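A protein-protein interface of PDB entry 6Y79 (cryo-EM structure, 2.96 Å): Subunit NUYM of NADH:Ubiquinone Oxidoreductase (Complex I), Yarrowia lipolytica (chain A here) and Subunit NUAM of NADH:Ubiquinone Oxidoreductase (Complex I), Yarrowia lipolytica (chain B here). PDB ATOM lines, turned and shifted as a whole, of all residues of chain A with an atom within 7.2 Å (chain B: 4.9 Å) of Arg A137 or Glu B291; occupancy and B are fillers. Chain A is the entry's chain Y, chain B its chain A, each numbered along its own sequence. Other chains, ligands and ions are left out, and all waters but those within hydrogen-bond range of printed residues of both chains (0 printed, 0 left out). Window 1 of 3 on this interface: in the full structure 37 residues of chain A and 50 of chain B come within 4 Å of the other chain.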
ATOM      1  N   LYS A  65      -7.300   8.949 -32.708  1.00  0.00           N
ATOM      2  CA  LYS A  65      -6.322   8.167 -31.971  1.00  0.00           C
ATOM      3  C   LYS A  65      -7.060   7.346 -30.929  1.00  0.00           C
ATOM      4  O   LYS A  65      -7.889   7.898 -30.195  1.00  0.00           O
ATOM      5  CB  LYS A  65      -5.293   9.073 -31.308  1.00  0.00           C
ATOM      6  CG  LYS A  65      -4.542   9.945 -32.288  1.00  0.00           C
ATOM      7  CD  LYS A  65      -3.538  10.834 -31.592  1.00  0.00           C
ATOM      8  CE  LYS A  65      -2.848  11.745 -32.591  1.00  0.00           C
ATOM      9  NZ  LYS A  65      -1.910  12.689 -31.927  1.00  0.00           N
ATOM     10  N   PRO A  66      -6.841   6.034 -30.873  1.00  0.00           N
ATOM     11  CA  PRO A  66      -7.611   5.203 -29.944  1.00  0.00           C
ATOM     12  C   PRO A  66      -7.235   5.497 -28.504  1.00  0.00           C
ATOM     13  O   PRO A  66      -6.068   5.728 -28.180  1.00  0.00           O
ATOM     14  CB  PRO A  66      -7.224   3.772 -30.340  1.00  0.00           C
ATOM     15  CG  PRO A  66      -6.639   3.892 -31.705  1.00  0.00           C
ATOM     16  CD  PRO A  66      -5.964   5.221 -31.727  1.00  0.00           C
ATOM     17  N   ALA A  67      -8.248   5.502 -27.638  1.00  0.00           N
ATOM     18  CA  ALA A  67      -7.988   5.601 -26.210  1.00  0.00           C
ATOM     19  C   ALA A  67      -7.407   4.312 -25.657  1.00  0.00           C
ATOM     20  O   ALA A  67      -6.878   4.312 -24.542  1.00  0.00           O
ATOM     21  CB  ALA A  67      -9.268   5.967 -25.461  1.00  0.00           C
ATOM     22  N   GLN A  69      -4.774   2.150 -27.014  1.00  0.00           N
ATOM     23  CA  GLN A  69      -3.330   2.015 -27.063  1.00  0.00           C
ATOM     24  C   GLN A  69      -2.681   3.311 -27.527  1.00  0.00           C
ATOM     25  O   GLN A  69      -3.345   4.222 -28.019  1.00  0.00           O
ATOM     26  CB  GLN A  69      -2.923   0.845 -27.968  1.00  0.00           C
ATOM     27  CG  GLN A  69      -3.624   0.808 -29.301  1.00  0.00           C
ATOM     28  CD  GLN A  69      -3.298  -0.441 -30.084  1.00  0.00           C
ATOM     29  OE1 GLN A  69      -2.437  -1.218 -29.694  1.00  0.00           O
ATOM     30  NE2 GLN A  69      -3.985  -0.637 -31.202  1.00  0.00           N
ATOM     31  N   SER A  70      -1.369   3.383 -27.347  1.00  0.00           N
ATOM     32  CA  SER A  70      -0.613   4.609 -27.529  1.00  0.00           C
ATOM     33  C   SER A  70      -0.118   4.800 -28.953  1.00  0.00           C
ATOM     34  O   SER A  70       0.699   5.693 -29.194  1.00  0.00           O
ATOM     35  CB  SER A  70       0.576   4.629 -26.567  1.00  0.00           C
ATOM     36  OG  SER A  70       0.132   4.599 -25.224  1.00  0.00           O
ATOM     37  N   GLU A  72      -0.385   5.713 -33.058  1.00  0.00           N
ATOM     38  CA  GLU A  72      -1.022   6.783 -33.815  1.00  0.00           C
ATOM     39  C   GLU A  72      -0.907   6.566 -35.317  1.00  0.00           C
ATOM     40  O   GLU A  72      -1.047   7.524 -36.081  1.00  0.00           O
ATOM     41  CB  GLU A  72      -0.416   8.139 -33.443  1.00  0.00           C
ATOM     42  CG  GLU A  72      -0.644   8.565 -32.001  1.00  0.00           C
ATOM     43  CD  GLU A  72       0.073   9.850 -31.638  1.00  0.00           C
ATOM     44  OE1 GLU A  72       0.786  10.403 -32.500  1.00  0.00           O
ATOM     45  OE2 GLU A  72      -0.065  10.303 -30.484  1.00  0.00           O
ATOM     46  N   HIS A 135      -8.982  16.538 -34.335  1.00  0.00           N
ATOM     47  CA  HIS A 135      -8.764  17.159 -33.033  1.00  0.00           C
ATOM     48  C   HIS A 135      -7.462  16.634 -32.451  1.00  0.00           C
ATOM     49  O   HIS A 135      -7.385  15.471 -32.045  1.00  0.00           O
ATOM     50  CB  HIS A 135      -9.934  16.897 -32.092  1.00  0.00           C
ATOM     51  CG  HIS A 135     -11.213  17.512 -32.555  1.00  0.00           C
ATOM     52  ND1 HIS A 135     -12.348  16.776 -32.816  1.00  0.00           N
ATOM     53  CD2 HIS A 135     -11.518  18.793 -32.866  1.00  0.00           C
ATOM     54  CE1 HIS A 135     -13.309  17.583 -33.228  1.00  0.00           C
ATOM     55  NE2 HIS A 135     -12.829  18.813 -33.270  1.00  0.00           N
ATOM     56  N   HIS A 136      -6.445  17.485 -32.412  1.00  0.00           N
ATOM     57  CA  HIS A 136      -5.158  17.115 -31.854  1.00  0.00           C
ATOM     58  C   HIS A 136      -5.105  17.499 -30.390  1.00  0.00           C
ATOM     59  O   HIS A 136      -5.990  18.167 -29.876  1.00  0.00           O
ATOM     60  CB  HIS A 136      -4.026  17.789 -32.614  1.00  0.00           C
ATOM     61  CG  HIS A 136      -3.903  17.333 -34.031  1.00  0.00           C
ATOM     62  ND1 HIS A 136      -3.363  16.113 -34.373  1.00  0.00           N
ATOM     63  CD2 HIS A 136      -4.259  17.928 -35.192  1.00  0.00           C
ATOM     64  CE1 HIS A 136      -3.388  15.978 -35.687  1.00  0.00           C
ATOM     65  NE2 HIS A 136      -3.926  17.065 -36.207  1.00  0.00           N
ATOM     66  N   ARG A 137      -4.039  17.092 -29.720  1.00  0.00           N
ATOM     67  CA  ARG A 137      -3.917  17.345 -28.296  1.00  0.00           C
ATOM     68  C   ARG A 137      -3.222  18.674 -28.040  1.00  0.00           C
ATOM     69  O   ARG A 137      -2.313  19.073 -28.770  1.00  0.00           O
ATOM     70  CB  ARG A 137      -3.155  16.203 -27.640  1.00  0.00           C
ATOM     71  CG  ARG A 137      -3.951  14.923 -27.590  1.00  0.00           C
ATOM     72  CD  ARG A 137      -3.058  13.780 -27.208  1.00  0.00           C
ATOM     73  NE  ARG A 137      -3.780  12.566 -26.901  1.00  0.00           N
ATOM     74  CZ  ARG A 137      -3.216  11.487 -26.382  1.00  0.00           C
ATOM     75  NH1 ARG A 137      -1.923  11.487 -26.114  1.00  0.00           N
ATOM     76  NH2 ARG A 137      -3.950  10.417 -26.109  1.00  0.00           N
ATOM     77  N   LYS A 138      -3.671  19.366 -26.996  1.00  0.00           N
ATOM     78  CA  LYS A 138      -3.061  20.630 -26.616  1.00  0.00           C
ATOM     79  C   LYS A 138      -1.705  20.367 -25.985  1.00  0.00           C
ATOM     80  O   LYS A 138      -1.579  19.517 -25.098  1.00  0.00           O
ATOM     81  CB  LYS A 138      -3.952  21.395 -25.641  1.00  0.00           C
ATOM     82  CG  LYS A 138      -3.428  22.779 -25.306  1.00  0.00           C
ATOM     83  CD  LYS A 138      -4.329  23.494 -24.326  1.00  0.00           C
ATOM     84  CE  LYS A 138      -4.240  22.868 -22.946  1.00  0.00           C
ATOM     85  NZ  LYS A 138      -2.891  23.017 -22.340  1.00  0.00           N
ATOM     86  N   PHE A 139      -0.691  21.088 -26.442  1.00  0.00           N
ATOM     87  CA  PHE A 139       0.635  20.908 -25.878  1.00  0.00           C
ATOM     88  C   PHE A 139       0.691  21.540 -24.496  1.00  0.00           C
ATOM     89  O   PHE A 139       0.387  22.726 -24.331  1.00  0.00           O
ATOM     90  CB  PHE A 139       1.704  21.508 -26.784  1.00  0.00           C
ATOM     91  CG  PHE A 139       3.086  21.248 -26.302  1.00  0.00           C
ATOM     92  CD1 PHE A 139       3.693  20.027 -26.572  1.00  0.00           C
ATOM     93  CD2 PHE A 139       3.775  22.184 -25.541  1.00  0.00           C
ATOM     94  CE1 PHE A 139       4.952  19.767 -26.119  1.00  0.00           C
ATOM     95  CE2 PHE A 139       5.029  21.910 -25.082  1.00  0.00           C
ATOM     96  CZ  PHE A 139       5.638  20.711 -25.361  1.00  0.00           C
ATOM     97  N   ARG A 140       1.107  20.752 -23.513  1.00  0.00           N
ATOM     98  CA  ARG A 140       1.309  21.211 -22.148  1.00  0.00           C
ATOM     99  C   ARG A 140       2.693  20.770 -21.701  1.00  0.00           C
ATOM    100  O   ARG A 140       3.080  19.622 -21.932  1.00  0.00           O
ATOM    101  CB  ARG A 140       0.234  20.646 -21.223  1.00  0.00           C
ATOM    102  CG  ARG A 140       0.320  21.131 -19.804  1.00  0.00           C
ATOM    103  CD  ARG A 140      -0.441  22.418 -19.633  1.00  0.00           C
ATOM    104  NE  ARG A 140      -0.286  22.961 -18.290  1.00  0.00           N
ATOM    105  CZ  ARG A 140      -0.821  24.106 -17.889  1.00  0.00           C
ATOM    106  NH1 ARG A 140      -0.627  24.532 -16.649  1.00  0.00           N
ATOM    107  NH2 ARG A 140      -1.547  24.827 -18.731  1.00  0.00           N
ATOM    108  N   HIS B  71       1.750   9.075 -20.207  1.00  0.00           N
ATOM    109  CA  HIS B  71       0.446   9.445 -20.724  1.00  0.00           C
ATOM    110  C   HIS B  71       0.338  10.960 -20.640  1.00  0.00           C
ATOM    111  O   HIS B  71       0.928  11.577 -19.750  1.00  0.00           O
ATOM    112  CB  HIS B  71      -0.665   8.744 -19.933  1.00  0.00           C
ATOM    113  CG  HIS B  71      -2.031   8.928 -20.506  1.00  0.00           C
ATOM    114  ND1 HIS B  71      -2.836   9.994 -20.173  1.00  0.00           N
ATOM    115  CD2 HIS B  71      -2.740   8.181 -21.383  1.00  0.00           C
ATOM    116  CE1 HIS B  71      -3.981   9.900 -20.823  1.00  0.00           C
ATOM    117  NE2 HIS B  71      -3.948   8.809 -21.565  1.00  0.00           N
ATOM    118  N   ASP B  72      -0.397  11.557 -21.592  1.00  0.00           N
ATOM    119  CA  ASP B  72      -0.490  13.015 -21.676  1.00  0.00           C
ATOM    120  C   ASP B  72      -1.199  13.604 -20.460  1.00  0.00           C
ATOM    121  O   ASP B  72      -0.774  14.629 -19.919  1.00  0.00           O
ATOM    122  CB  ASP B  72      -1.208  13.423 -22.966  1.00  0.00           C
ATOM    123  CG  ASP B  72      -1.095  14.925 -23.281  1.00  0.00           C
ATOM    124  OD1 ASP B  72      -0.447  15.693 -22.537  1.00  0.00           O
ATOM    125  OD2 ASP B  72      -1.670  15.350 -24.304  1.00  0.00           O
ATOM    126  N   LYS B  73      -2.298  12.975 -20.036  1.00  0.00           N
ATOM    127  CA  LYS B  73      -3.118  13.539 -18.929  1.00  0.00           C
ATOM    128  C   LYS B  73      -2.678  13.011 -17.558  1.00  0.00           C
ATOM    129  O   LYS B  73      -3.478  13.137 -16.613  1.00  0.00           O
ATOM    130  CB  LYS B  73      -4.593  13.203 -19.175  1.00  0.00           C
ATOM    131  CG  LYS B  73      -5.090  13.489 -20.585  1.00  0.00           C
ATOM    132  CD  LYS B  73      -4.875  14.924 -21.013  1.00  0.00           C
ATOM    133  CE  LYS B  73      -5.233  15.173 -22.464  1.00  0.00           C
ATOM    134  NZ  LYS B  73      -4.395  14.365 -23.382  1.00  0.00           N
ATOM    135  N   PRO B 282     -13.856   7.006 -25.188  1.00  0.00           N
ATOM    136  CA  PRO B 282     -13.761   8.432 -25.529  1.00  0.00           C
ATOM    137  C   PRO B 282     -12.692   8.715 -26.581  1.00  0.00           C
ATOM    138  O   PRO B 282     -11.554   8.257 -26.470  1.00  0.00           O
ATOM    139  CB  PRO B 282     -13.413   9.092 -24.192  1.00  0.00           C
ATOM    140  CG  PRO B 282     -12.687   8.027 -23.455  1.00  0.00           C
ATOM    141  CD  PRO B 282     -13.282   6.729 -23.859  1.00  0.00           C
ATOM    142  N   VAL B 284     -10.618  11.996 -28.231  1.00  0.00           N
ATOM    143  CA  VAL B 284     -10.067  13.145 -27.524  1.00  0.00           C
ATOM    144  C   VAL B 284     -10.638  14.441 -28.095  1.00  0.00           C
ATOM    145  O   VAL B 284     -10.874  14.574 -29.302  1.00  0.00           O
ATOM    146  CB  VAL B 284      -8.522  13.111 -27.564  1.00  0.00           C
ATOM    147  CG1 VAL B 284      -7.967  13.254 -28.981  1.00  0.00           C
ATOM    148  CG2 VAL B 284      -7.905  14.137 -26.612  1.00  0.00           C
ATOM    149  N   HIS B 285     -10.947  15.370 -27.191  1.00  0.00           N
ATOM    150  CA  HIS B 285     -11.209  16.766 -27.516  1.00  0.00           C
ATOM    151  C   HIS B 285     -10.800  17.562 -26.290  1.00  0.00           C
ATOM    152  O   HIS B 285     -11.330  17.323 -25.202  1.00  0.00           O
ATOM    153  CB  HIS B 285     -12.675  17.014 -27.850  1.00  0.00           C
ATOM    154  CG  HIS B 285     -12.978  18.418 -28.282  1.00  0.00           C
ATOM    155  ND1 HIS B 285     -12.646  18.899 -29.528  1.00  0.00           N
ATOM    156  CD2 HIS B 285     -13.582  19.443 -27.638  1.00  0.00           C
ATOM    157  CE1 HIS B 285     -13.032  20.157 -29.634  1.00  0.00           C
ATOM    158  NE2 HIS B 285     -13.609  20.510 -28.502  1.00  0.00           N
ATOM    159  N   GLU B 286      -9.865  18.494 -26.459  1.00  0.00           N
ATOM    160  CA  GLU B 286      -9.295  19.179 -25.307  1.00  0.00           C
ATOM    161  C   GLU B 286     -10.245  20.181 -24.667  1.00  0.00           C
ATOM    162  O   GLU B 286      -9.962  20.654 -23.562  1.00  0.00           O
ATOM    163  CB  GLU B 286      -7.998  19.876 -25.707  1.00  0.00           C
ATOM    164  CG  GLU B 286      -6.899  18.907 -26.089  1.00  0.00           C
ATOM    165  CD  GLU B 286      -6.438  18.045 -24.924  1.00  0.00           C
ATOM    166  OE1 GLU B 286      -6.447  18.528 -23.771  1.00  0.00           O
ATOM    167  OE2 GLU B 286      -6.069  16.877 -25.163  1.00  0.00           O
ATOM    168  N   ASN B 289     -14.244  17.311 -23.069  1.00  0.00           N
ATOM    169  CA  ASN B 289     -14.098  16.263 -22.071  1.00  0.00           C
ATOM    170  C   ASN B 289     -12.670  15.997 -21.655  1.00  0.00           C
ATOM    171  O   ASN B 289     -12.468  15.471 -20.552  1.00  0.00           O
ATOM    172  CB  ASN B 289     -14.742  14.945 -22.545  1.00  0.00           C
ATOM    173  CG  ASN B 289     -14.131  14.372 -23.829  1.00  0.00           C
ATOM    174  OD1 ASN B 289     -13.155  14.875 -24.375  1.00  0.00           O
ATOM    175  ND2 ASN B 289     -14.727  13.286 -24.306  1.00  0.00           N
ATOM    176  N   GLU B 290     -11.691  16.340 -22.498  1.00  0.00           N
ATOM    177  CA  GLU B 290     -10.263  16.152 -22.251  1.00  0.00           C
ATOM    178  C   GLU B 290      -9.969  14.679 -21.958  1.00  0.00           C
ATOM    179  O   GLU B 290      -9.604  14.307 -20.850  1.00  0.00           O
ATOM    180  CB  GLU B 290      -9.794  17.086 -21.122  1.00  0.00           C
ATOM    181  CG  GLU B 290      -8.315  17.198 -20.894  1.00  0.00           C
ATOM    182  CD  GLU B 290      -7.997  18.138 -19.764  1.00  0.00           C
ATOM    183  OE1 GLU B 290      -8.930  18.777 -19.254  1.00  0.00           O
ATOM    184  OE2 GLU B 290      -6.818  18.218 -19.353  1.00  0.00           O
ATOM    185  N   GLU B 291     -10.326  13.829 -22.930  1.00  0.00           N
ATOM    186  CA  GLU B 291     -10.036  12.393 -23.000  1.00  0.00           C
ATOM    187  C   GLU B 291     -10.777  11.553 -21.947  1.00  0.00           C
ATOM    188  O   GLU B 291     -10.859  10.330 -22.073  1.00  0.00           O
ATOM    189  CB  GLU B 291      -8.506  12.177 -22.913  1.00  0.00           C
ATOM    190  CG  GLU B 291      -7.971  10.764 -23.169  1.00  0.00           C
ATOM    191  CD  GLU B 291      -6.468  10.660 -23.054  1.00  0.00           C
ATOM    192  OE1 GLU B 291      -5.811  11.695 -22.830  1.00  0.00           O
ATOM    193  OE2 GLU B 291      -5.945   9.531 -23.171  1.00  0.00           O
ATOM    194  N   TRP B 292     -11.433  12.174 -20.971  1.00  0.00           N
ATOM    195  CA  TRP B 292     -11.984  11.443 -19.838  1.00  0.00           C
ATOM    196  C   TRP B 292     -13.500  11.582 -19.846  1.00  0.00           C
ATOM    197  O   TRP B 292     -14.024  12.679 -20.057  1.00  0.00           O
ATOM    198  CB  TRP B 292     -11.361  11.934 -18.522  1.00  0.00           C
ATOM    199  CG  TRP B 292      -9.896  11.621 -18.446  1.00  0.00           C
ATOM    200  CD1 TRP B 292      -8.852  12.477 -18.648  1.00  0.00           C
ATOM    201  CD2 TRP B 292      -9.311  10.346 -18.197  1.00  0.00           C
ATOM    202  NE1 TRP B 292      -7.661  11.816 -18.536  1.00  0.00           N
ATOM    203  CE2 TRP B 292      -7.915  10.502 -18.260  1.00  0.00           C
ATOM    204  CE3 TRP B 292      -9.832   9.086 -17.941  1.00  0.00           C
ATOM    205  CZ2 TRP B 292      -7.040   9.440 -18.062  1.00  0.00           C
ATOM    206  CZ3 TRP B 292      -8.969   8.033 -17.740  1.00  0.00           C
ATOM    207  CH2 TRP B 292      -7.595   8.214 -17.798  1.00  0.00           C
ATOM    208  N   ILE B 293     -14.201  10.467 -19.623  1.00  0.00           N
ATOM    209  CA  ILE B 293     -15.626  10.368 -19.905  1.00  0.00           C
ATOM    210  C   ILE B 293     -16.350   9.791 -18.686  1.00  0.00           C
ATOM    211  O   ILE B 293     -15.758   9.129 -17.837  1.00  0.00           O
ATOM    212  CB  ILE B 293     -15.870   9.519 -21.180  1.00  0.00           C
ATOM    213  CG1 ILE B 293     -17.257   9.724 -21.780  1.00  0.00           C
ATOM    214  CG2 ILE B 293     -15.659   8.050 -20.935  1.00  0.00           C
ATOM    215  CD1 ILE B 293     -17.409   9.008 -23.059  1.00  0.00           C
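The side-chain carboxylate (OE2) of Glu B291 lies within salt-bridge range of the guanidinium group (NH2) of Arg A137 (3.7 Å).
The side-chain amide oxygen (OD1) of Asn B289 sits close to the backbone carbonyl oxygen (O) of His B285.
OE2 of Glu B286 is in salt-bridge range of NZ of Lys B73 (3.5 Å).
NZ of Lys B73 lies within salt-bridge range of OE1 of Glu B291, 3.1 Å away.
The side-chain carboxylate (OD2) of Asp B72 lies within salt-bridge range of the side-chain amino group (NZ) of Lys B73, 3.0 Å away.
The side-chain amide oxygen of Asn B289 sits at hydrogen-bond distance from the backbone NH of Glu B291, at 3.3 Å.
O of His B285 is in hydrogen-bond range of N of Glu B290.
Among the printed residues, merely in contact across the chains: Lys A138 with Glu B286, Ala A67 with Pro B282, His A135 with His B285, Arg A137 with Asp B72, His A135 with Val B284, Arg A137 with Glu B286, His A136 with Glu B286 and Arg A137 with Lys B73.
Hydrophobic or aromatic side chains of chain B that line the printed part of chain A: Val B284 and His B285.
Printed residues of chain B within 4 Å of Arg A137: Asp B72, Lys B73, Glu B286 and Glu B291.
Of the printed residues of chain A, Glu B291 touches Arg A137.
Printed residues of chain B within 4 Å of Lys A138: Glu B286 (3.4 Å).
Of the printed residues of chain A, Val B284 touches His A135.
Printed residues of chain B within 4 Å of His A135: Val B284 and His B285.
The nearest printed residue of chain B that does not touch Arg A137 is Val B284 (4.1 Å).
The nearest printed residue of chain B that does not touch His A135 is Glu B286 (5.9 Å).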
